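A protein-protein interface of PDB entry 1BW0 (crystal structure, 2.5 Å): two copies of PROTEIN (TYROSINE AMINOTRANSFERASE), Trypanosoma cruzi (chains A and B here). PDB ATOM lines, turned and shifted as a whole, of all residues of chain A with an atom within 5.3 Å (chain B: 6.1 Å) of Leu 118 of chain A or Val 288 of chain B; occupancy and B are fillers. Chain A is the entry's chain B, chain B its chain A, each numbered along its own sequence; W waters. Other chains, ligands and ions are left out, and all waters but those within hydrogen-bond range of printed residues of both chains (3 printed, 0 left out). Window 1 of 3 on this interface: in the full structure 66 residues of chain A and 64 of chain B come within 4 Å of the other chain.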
ATOM      1  N   SER A 111      17.044 -15.312  10.789  1.00  0.00           N
ATOM      2  CA  SER A 111      16.172 -15.886   9.761  1.00  0.00           C
ATOM      3  C   SER A 111      15.665 -14.847   8.778  1.00  0.00           C
ATOM      4  O   SER A 111      14.496 -14.467   8.742  1.00  0.00           O
ATOM      5  CB  SER A 111      15.032 -16.583  10.504  1.00  0.00           C
ATOM      6  OG  SER A 111      14.143 -17.233   9.636  1.00  0.00           O
ATOM      7  N   GLY A 113      16.066 -10.970   6.692  1.00  0.00           N
ATOM      8  CA  GLY A 113      16.057  -9.588   7.113  1.00  0.00           C
ATOM      9  C   GLY A 113      14.991  -9.268   8.145  1.00  0.00           C
ATOM     10  O   GLY A 113      15.307  -8.643   9.167  1.00  0.00           O
ATOM     11  N   SER A 114      13.746  -9.671   7.919  1.00  0.00           N
ATOM     12  CA  SER A 114      12.640  -9.402   8.820  1.00  0.00           C
ATOM     13  C   SER A 114      12.937  -9.793  10.262  1.00  0.00           C
ATOM     14  O   SER A 114      12.661  -9.036  11.195  1.00  0.00           O
ATOM     15  CB  SER A 114      11.352 -10.122   8.389  1.00  0.00           C
ATOM     16  OG  SER A 114      10.802  -9.547   7.219  1.00  0.00           O
ATOM     17  N   HIS A 115      13.491 -10.986  10.452  1.00  0.00           N
ATOM     18  CA  HIS A 115      13.863 -11.456  11.788  1.00  0.00           C
ATOM     19  C   HIS A 115      14.991 -10.595  12.351  1.00  0.00           C
ATOM     20  O   HIS A 115      14.979 -10.192  13.518  1.00  0.00           O
ATOM     21  CB  HIS A 115      14.236 -12.929  11.704  1.00  0.00           C
ATOM     22  CG  HIS A 115      14.579 -13.570  13.012  1.00  0.00           C
ATOM     23  ND1 HIS A 115      15.543 -14.541  13.131  1.00  0.00           N
ATOM     24  CD2 HIS A 115      14.078 -13.371  14.253  1.00  0.00           C
ATOM     25  CE1 HIS A 115      15.618 -14.908  14.402  1.00  0.00           C
ATOM     26  NE2 HIS A 115      14.740 -14.212  15.103  1.00  0.00           N
ATOM     27  N   GLY A 116      15.964 -10.270  11.499  1.00  0.00           N
ATOM     28  CA  GLY A 116      17.074  -9.421  11.891  1.00  0.00           C
ATOM     29  C   GLY A 116      16.566  -8.076  12.415  1.00  0.00           C
ATOM     30  O   GLY A 116      17.032  -7.598  13.451  1.00  0.00           O
ATOM     31  N   ILE A 117      15.577  -7.468  11.749  1.00  0.00           N
ATOM     32  CA  ILE A 117      15.023  -6.199  12.208  1.00  0.00           C
ATOM     33  C   ILE A 117      14.325  -6.368  13.553  1.00  0.00           C
ATOM     34  O   ILE A 117      14.520  -5.556  14.475  1.00  0.00           O
ATOM     35  CB  ILE A 117      14.097  -5.571  11.157  1.00  0.00           C
ATOM     36  CG1 ILE A 117      14.918  -5.273   9.899  1.00  0.00           C
ATOM     37  CG2 ILE A 117      13.428  -4.321  11.699  1.00  0.00           C
ATOM     38  CD1 ILE A 117      14.098  -4.950   8.677  1.00  0.00           C
ATOM     39  N   LEU A 118      13.548  -7.441  13.688  1.00  0.00           N
ATOM     40  CA  LEU A 118      12.871  -7.719  14.954  1.00  0.00           C
ATOM     41  C   LEU A 118      13.854  -7.781  16.120  1.00  0.00           C
ATOM     42  O   LEU A 118      13.674  -7.155  17.162  1.00  0.00           O
ATOM     43  CB  LEU A 118      12.083  -9.022  14.841  1.00  0.00           C
ATOM     44  CG  LEU A 118      11.417  -9.549  16.114  1.00  0.00           C
ATOM     45  CD1 LEU A 118      10.466  -8.504  16.678  1.00  0.00           C
ATOM     46  CD2 LEU A 118      10.667 -10.832  15.812  1.00  0.00           C
ATOM     47  N   MET A 119      14.936  -8.527  15.971  1.00  0.00           N
ATOM     48  CA  MET A 119      15.968  -8.652  16.987  1.00  0.00           C
ATOM     49  C   MET A 119      16.619  -7.308  17.295  1.00  0.00           C
ATOM     50  O   MET A 119      16.695  -6.949  18.474  1.00  0.00           O
ATOM     51  CB  MET A 119      17.005  -9.692  16.569  1.00  0.00           C
ATOM     52  CG  MET A 119      16.512 -11.131  16.561  1.00  0.00           C
ATOM     53  SD  MET A 119      17.560 -12.215  15.570  1.00  0.00           S
ATOM     54  CE  MET A 119      19.117 -12.080  16.450  1.00  0.00           C
ATOM     55  N   ALA A 120      17.047  -6.541  16.300  1.00  0.00           N
ATOM     56  CA  ALA A 120      17.681  -5.253  16.524  1.00  0.00           C
ATOM     57  C   ALA A 120      16.811  -4.267  17.295  1.00  0.00           C
ATOM     58  O   ALA A 120      17.302  -3.703  18.274  1.00  0.00           O
ATOM     59  CB  ALA A 120      18.107  -4.584  15.222  1.00  0.00           C
ATOM     60  N   ILE A 121      15.572  -4.045  16.855  1.00  0.00           N
ATOM     61  CA  ILE A 121      14.684  -3.117  17.539  1.00  0.00           C
ATOM     62  C   ILE A 121      14.285  -3.572  18.936  1.00  0.00           C
ATOM     63  O   ILE A 121      14.248  -2.720  19.839  1.00  0.00           O
ATOM     64  CB  ILE A 121      13.415  -2.828  16.715  1.00  0.00           C
ATOM     65  CG1 ILE A 121      13.796  -2.110  15.414  1.00  0.00           C
ATOM     66  CG2 ILE A 121      12.402  -1.992  17.487  1.00  0.00           C
ATOM     67  CD1 ILE A 121      12.647  -1.996  14.430  1.00  0.00           C
ATOM     68  N   THR A 122      13.977  -4.849  19.150  1.00  0.00           N
ATOM     69  CA  THR A 122      13.538  -5.278  20.477  1.00  0.00           C
ATOM     70  C   THR A 122      14.636  -5.597  21.473  1.00  0.00           C
ATOM     71  O   THR A 122      14.383  -5.778  22.666  1.00  0.00           O
ATOM     72  CB  THR A 122      12.607  -6.502  20.377  1.00  0.00           C
ATOM     73  OG1 THR A 122      13.349  -7.579  19.796  1.00  0.00           O
ATOM     74  CG2 THR A 122      11.380  -6.152  19.559  1.00  0.00           C
ATOM     75  N   ALA A 123      15.885  -5.640  21.029  1.00  0.00           N
ATOM     76  CA  ALA A 123      17.044  -5.901  21.852  1.00  0.00           C
ATOM     77  C   ALA A 123      17.416  -4.668  22.674  1.00  0.00           C
ATOM     78  O   ALA A 123      18.104  -4.787  23.687  1.00  0.00           O
ATOM     79  CB  ALA A 123      18.248  -6.237  20.981  1.00  0.00           C
ATOM     80  N   HIS A 140       8.661  -2.933   7.520  1.00  0.00           N
ATOM     81  CA  HIS A 140       8.932  -3.802   8.655  1.00  0.00           C
ATOM     82  C   HIS A 140       9.388  -3.097   9.925  1.00  0.00           C
ATOM     83  O   HIS A 140       9.062  -3.579  11.022  1.00  0.00           O
ATOM     84  CB  HIS A 140       9.903  -4.937   8.303  1.00  0.00           C
ATOM     85  CG  HIS A 140       9.595  -6.146   9.142  1.00  0.00           C
ATOM     86  ND1 HIS A 140       8.438  -6.871   8.961  1.00  0.00           N
ATOM     87  CD2 HIS A 140      10.274  -6.752  10.145  1.00  0.00           C
ATOM     88  CE1 HIS A 140       8.428  -7.883   9.821  1.00  0.00           C
ATOM     89  NE2 HIS A 140       9.523  -7.828  10.558  1.00  0.00           N
ATOM     90  N   VAL A 144       7.364  -3.995  13.349  1.00  0.00           N
ATOM     91  CA  VAL A 144       7.966  -4.424  14.601  1.00  0.00           C
ATOM     92  C   VAL A 144       7.694  -3.397  15.700  1.00  0.00           C
ATOM     93  O   VAL A 144       7.367  -3.774  16.825  1.00  0.00           O
ATOM     94  CB  VAL A 144       9.483  -4.654  14.452  1.00  0.00           C
ATOM     95  CG1 VAL A 144      10.150  -4.909  15.796  1.00  0.00           C
ATOM     96  CG2 VAL A 144       9.770  -5.819  13.521  1.00  0.00           C
ATOM     97  N   TYR A 148       5.250  -3.940  19.356  1.00  0.00           N
ATOM     98  CA  TYR A 148       5.862  -3.983  20.682  1.00  0.00           C
ATOM     99  C   TYR A 148       5.610  -2.703  21.462  1.00  0.00           C
ATOM    100  O   TYR A 148       6.221  -2.458  22.507  1.00  0.00           O
ATOM    101  CB  TYR A 148       7.371  -4.226  20.580  1.00  0.00           C
ATOM    102  CG  TYR A 148       7.723  -5.658  20.255  1.00  0.00           C
ATOM    103  CD1 TYR A 148       7.557  -6.185  18.979  1.00  0.00           C
ATOM    104  CD2 TYR A 148       8.214  -6.496  21.252  1.00  0.00           C
ATOM    105  CE1 TYR A 148       7.875  -7.501  18.705  1.00  0.00           C
ATOM    106  CE2 TYR A 148       8.519  -7.819  20.985  1.00  0.00           C
ATOM    107  CZ  TYR A 148       8.354  -8.316  19.708  1.00  0.00           C
ATOM    108  OH  TYR A 148       8.680  -9.627  19.456  1.00  0.00           O
ATOM    109  N   ARG A 261      15.731 -17.700   3.814  1.00  0.00           N
ATOM    110  CA  ARG A 261      15.684 -17.075   5.109  1.00  0.00           C
ATOM    111  C   ARG A 261      17.028 -17.051   5.828  1.00  0.00           C
ATOM    112  O   ARG A 261      17.142 -17.542   6.951  1.00  0.00           O
ATOM    113  CB  ARG A 261      14.609 -17.694   6.013  1.00  0.00           C
ATOM    114  CG  ARG A 261      13.227 -17.814   5.390  1.00  0.00           C
ATOM    115  CD  ARG A 261      12.725 -16.547   4.712  1.00  0.00           C
ATOM    116  NE  ARG A 261      12.702 -15.407   5.613  1.00  0.00           N
ATOM    117  CZ  ARG A 261      12.781 -14.118   5.310  1.00  0.00           C
ATOM    118  NH1 ARG A 261      12.895 -13.685   4.057  1.00  0.00           N
ATOM    119  NH2 ARG A 261      12.739 -13.222   6.294  1.00  0.00           N
ATOM    120  N   VAL A 284      17.477 -12.112  22.545  1.00  0.00           N
ATOM    121  CA  VAL A 284      16.300 -12.111  21.691  1.00  0.00           C
ATOM    122  C   VAL A 284      16.292 -13.245  20.683  1.00  0.00           C
ATOM    123  O   VAL A 284      15.254 -13.842  20.387  1.00  0.00           O
ATOM    124  CB  VAL A 284      16.174 -10.742  20.990  1.00  0.00           C
ATOM    125  CG1 VAL A 284      15.172 -10.725  19.853  1.00  0.00           C
ATOM    126  CG2 VAL A 284      15.733  -9.716  22.031  1.00  0.00           C
ATOM    127  N   VAL A 288      13.803 -17.680  18.923  1.00  0.00           N
ATOM    128  CA  VAL A 288      13.530 -18.348  17.651  1.00  0.00           C
ATOM    129  C   VAL A 288      14.552 -19.417  17.325  1.00  0.00           C
ATOM    130  O   VAL A 288      14.208 -20.479  16.800  1.00  0.00           O
ATOM    131  CB  VAL A 288      13.354 -17.322  16.519  1.00  0.00           C
ATOM    132  CG1 VAL A 288      13.131 -17.992  15.168  1.00  0.00           C
ATOM    133  CG2 VAL A 288      12.178 -16.391  16.800  1.00  0.00           C
ATOM    134  N   SER B 111       9.433 -21.621  12.162  1.00  0.00           N
ATOM    135  CA  SER B 111      10.864 -21.896  12.191  1.00  0.00           C
ATOM    136  C   SER B 111      11.255 -22.794  13.363  1.00  0.00           C
ATOM    137  O   SER B 111      11.918 -22.399  14.326  1.00  0.00           O
ATOM    138  CB  SER B 111      11.617 -20.562  12.226  1.00  0.00           C
ATOM    139  OG  SER B 111      13.023 -20.712  12.137  1.00  0.00           O
ATOM    140  N   HIS B 115       9.974 -21.517  17.721  1.00  0.00           N
ATOM    141  CA  HIS B 115       9.193 -20.453  17.110  1.00  0.00           C
ATOM    142  C   HIS B 115       7.690 -20.701  17.248  1.00  0.00           C
ATOM    143  O   HIS B 115       6.894 -19.806  17.566  1.00  0.00           O
ATOM    144  CB  HIS B 115       9.543 -20.312  15.623  1.00  0.00           C
ATOM    145  CG  HIS B 115       8.961 -19.078  15.007  1.00  0.00           C
ATOM    146  ND1 HIS B 115       8.601 -18.998  13.679  1.00  0.00           N
ATOM    147  CD2 HIS B 115       8.669 -17.872  15.565  1.00  0.00           C
ATOM    148  CE1 HIS B 115       8.131 -17.785  13.443  1.00  0.00           C
ATOM    149  NE2 HIS B 115       8.157 -17.084  14.566  1.00  0.00           N
ATOM    150  N   LEU B 118       6.712 -19.914  20.784  1.00  0.00           N
ATOM    151  CA  LEU B 118       6.702 -18.457  20.896  1.00  0.00           C
ATOM    152  C   LEU B 118       5.427 -17.883  20.278  1.00  0.00           C
ATOM    153  O   LEU B 118       4.762 -17.065  20.915  1.00  0.00           O
ATOM    154  CB  LEU B 118       7.964 -17.861  20.274  1.00  0.00           C
ATOM    155  CG  LEU B 118       7.916 -16.392  19.852  1.00  0.00           C
ATOM    156  CD1 LEU B 118       7.746 -15.483  21.058  1.00  0.00           C
ATOM    157  CD2 LEU B 118       9.168 -15.998  19.087  1.00  0.00           C
ATOM    158  N   VAL B 284       1.243 -13.039  14.361  1.00  0.00           N
ATOM    159  CA  VAL B 284       2.567 -13.175  14.971  1.00  0.00           C
ATOM    160  C   VAL B 284       3.588 -13.749  14.007  1.00  0.00           C
ATOM    161  O   VAL B 284       4.739 -13.326  14.016  1.00  0.00           O
ATOM    162  CB  VAL B 284       2.499 -13.983  16.281  1.00  0.00           C
ATOM    163  CG1 VAL B 284       3.877 -14.379  16.783  1.00  0.00           C
ATOM    164  CG2 VAL B 284       1.802 -13.157  17.359  1.00  0.00           C
ATOM    165  N   GLY B 285       3.186 -14.638  13.101  1.00  0.00           N
ATOM    166  CA  GLY B 285       4.089 -15.212  12.120  1.00  0.00           C
ATOM    167  C   GLY B 285       4.620 -14.164  11.155  1.00  0.00           C
ATOM    168  O   GLY B 285       5.696 -14.354  10.579  1.00  0.00           O
ATOM    169  N   MET B 286       3.919 -13.048  10.975  1.00  0.00           N
ATOM    170  CA  MET B 286       4.321 -11.960  10.110  1.00  0.00           C
ATOM    171  C   MET B 286       5.519 -11.175  10.627  1.00  0.00           C
ATOM    172  O   MET B 286       6.069 -10.356   9.890  1.00  0.00           O
ATOM    173  CB  MET B 286       3.153 -11.004   9.859  1.00  0.00           C
ATOM    174  CG  MET B 286       2.041 -11.581   9.007  1.00  0.00           C
ATOM    175  SD  MET B 286       0.932 -10.318   8.350  1.00  0.00           S
ATOM    176  CE  MET B 286       0.127  -9.749   9.849  1.00  0.00           C
ATOM    177  N   LEU B 287       5.956 -11.352  11.857  1.00  0.00           N
ATOM    178  CA  LEU B 287       7.115 -10.685  12.416  1.00  0.00           C
ATOM    179  C   LEU B 287       8.400 -11.347  11.927  1.00  0.00           C
ATOM    180  O   LEU B 287       9.387 -10.675  11.635  1.00  0.00           O
ATOM    181  CB  LEU B 287       7.056 -10.696  13.954  1.00  0.00           C
ATOM    182  CG  LEU B 287       5.867  -9.947  14.569  1.00  0.00           C
ATOM    183  CD1 LEU B 287       5.651 -10.309  16.031  1.00  0.00           C
ATOM    184  CD2 LEU B 287       6.038  -8.435  14.433  1.00  0.00           C
ATOM    185  N   VAL B 288       8.400 -12.668  11.837  1.00  0.00           N
ATOM    186  CA  VAL B 288       9.568 -13.442  11.424  1.00  0.00           C
ATOM    187  C   VAL B 288       9.521 -13.848   9.958  1.00  0.00           C
ATOM    188  O   VAL B 288      10.541 -13.955   9.273  1.00  0.00           O
ATOM    189  CB  VAL B 288       9.701 -14.664  12.360  1.00  0.00           C
ATOM    190  CG1 VAL B 288      10.701 -15.690  11.872  1.00  0.00           C
ATOM    191  CG2 VAL B 288      10.106 -14.188  13.756  1.00  0.00           C
ATOM    192  N   CYS B 289       8.340 -14.124   9.431  1.00  0.00           N
ATOM    193  CA  CYS B 289       8.092 -14.507   8.058  1.00  0.00           C
ATOM    194  C   CYS B 289       8.425 -15.910   7.603  1.00  0.00           C
ATOM    195  O   CYS B 289       8.942 -16.125   6.501  1.00  0.00           O
ATOM    196  CB  CYS B 289       8.731 -13.460   7.119  1.00  0.00           C
ATOM    197  SG  CYS B 289       7.863 -11.875   7.325  1.00  0.00           S
ATOM    198  N   GLY B 290       8.055 -16.925   8.375  1.00  0.00           N
ATOM    199  CA  GLY B 290       8.183 -18.301   8.017  1.00  0.00           C
ATOM    200  C   GLY B 290       9.538 -18.922   7.791  1.00  0.00           C
ATOM    201  O   GLY B 290      10.588 -18.285   7.739  1.00  0.00           O
HETATM  202  O   HOH W   1      14.857 -21.490  14.382  1.00  0.00           O
HETATM  203  O   HOH W   2      12.036 -16.080   8.411  1.00  0.00           O
HETATM  204  O   HOH W   3      14.118 -20.198   9.637  1.00  0.00           O
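Leu 118 of chain A touches Val 288 of chain B, and with the chains exchanged Val 288 of chain A touches Leu 118 of chain B. Val 288 of chain A touches Ser 111 of chain B, but with the chains exchanged Ser 111 of chain A does not touch Val 288 of chain B (4.02 Å). Positions printed for both chains: 111, 115, 118, 284 and 288. Of the 10 pairs that touch across the chains among the printed residues, 2 have their exchanged pair printed and touching as well.
Of the 18 printed residues of chain A, 5 touch a printed residue of chain B. Hydrophobic or aromatic side chains of chain A that line the printed part of chain B: Leu 118, His 140 and Val 288. Among the printed residues, 10 pairs touch across the chains. Among the printed residues, no Asp or Glu carboxylate lies within 4 Å of a Lys or Arg side-chain nitrogen of the other chain.
Of chain B, only Val 288 comes within 4 Å of Leu 118 of chain A. Ile 121 of chain A touches none of the printed residues of chain B. Of the printed residues of chain B, Arg 261 of chain A touches Val 288, Cys 289 and Gly 290. Of the printed residues of chain B, Val 288 of chain A touches Ser 111 and Leu 118. Of the printed residues of chain A, Leu 118 of chain B touches Val 288 (3.8 Å). Of the printed residues of chain A, Met 286 of chain B touches His 140 (3.4 Å). Of the printed residues of chain A, Val 288 of chain B touches Leu 118 (3.98 Å) and Arg 261 (3.8 Å). Of the printed residues of chain A, Cys 289 of chain B touches Ser 114 (3.8 Å) and Arg 261 (3.9 Å). The nearest residue of chain B that does not touch Leu 118 of chain A is Leu 287 of chain B (4.1 Å).
ND1 of His 115 of chain B is in hydrogen-bond range of N of Ser 111 of chain B (3.1 Å). O of Met 286 of chain B is in hydrogen-bond range of SG of Cys 289 of chain B, at 3.5 Å. NH2 of Arg 261 of chain A lies within hydrogen-bond range of O of Ser 111 of chain A (3.3 Å). NE2 of His 140 of chain A lies within hydrogen-bond range of O of Ser 114 of chain A, at 3.4 Å. The backbone carbonyl oxygen of Leu 118 of chain A lies within hydrogen-bond range of the side-chain hydroxyl of Thr 122 of chain A (2.7 Å).
Water W2 lies within hydrogen-bond range of the side-chain hydroxyl (OG) of Ser 111 of chain A (2.7 Å), the backbone carbonyl oxygen (O) of Gly 290 of chain B (2.7 Å), the backbone carbonyl oxygen (O) of Val 288 of chain B (2.7 Å) and the guanidinium group (NE) of Arg 261 of chain A (3.0 Å). Water W1 bridges the backbone carbonyl oxygen of Val 288 of chain A and the side-chain hydroxyl of Ser 111 of chain B. Water W3 lies within hydrogen-bond range of the side-chain hydroxyl (OG) of Ser 111 of chain B (2.8 Å) and the side-chain hydroxyl (OG) of Ser 111 of chain A (3.0 Å).
Ser 114 of chain A touches Leu 287 of chain B (O to O, 3.7 Å). CD2 of Leu 118 of chain A touches CG2 of Val 288 of chain B, 3.98 Å away. CE1 of His 140 of chain A touches O of Met 286 of chain B, 3.4 Å away. Arg 261 of chain A touches Val 288 of chain B. Cys 289 of chain B touches Arg 261 of chain A. Gly 290 of chain B touches Arg 261 of chain A. Val 288 of chain A touches Ser 111 of chain B. Leu 118 of chain B touches Val 288 of chain A (CD2 to CG2, 3.8 Å).
The backbone carbonyl oxygen of Leu 287 of chain B sits at hydrogen-bond distance from a ring nitrogen (NE2) of His 140 of chain A (3.0 Å). SG of Cys 289 of chain B lies within hydrogen-bond range of OG of Ser 114 of chain A, 3.8 Å away.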
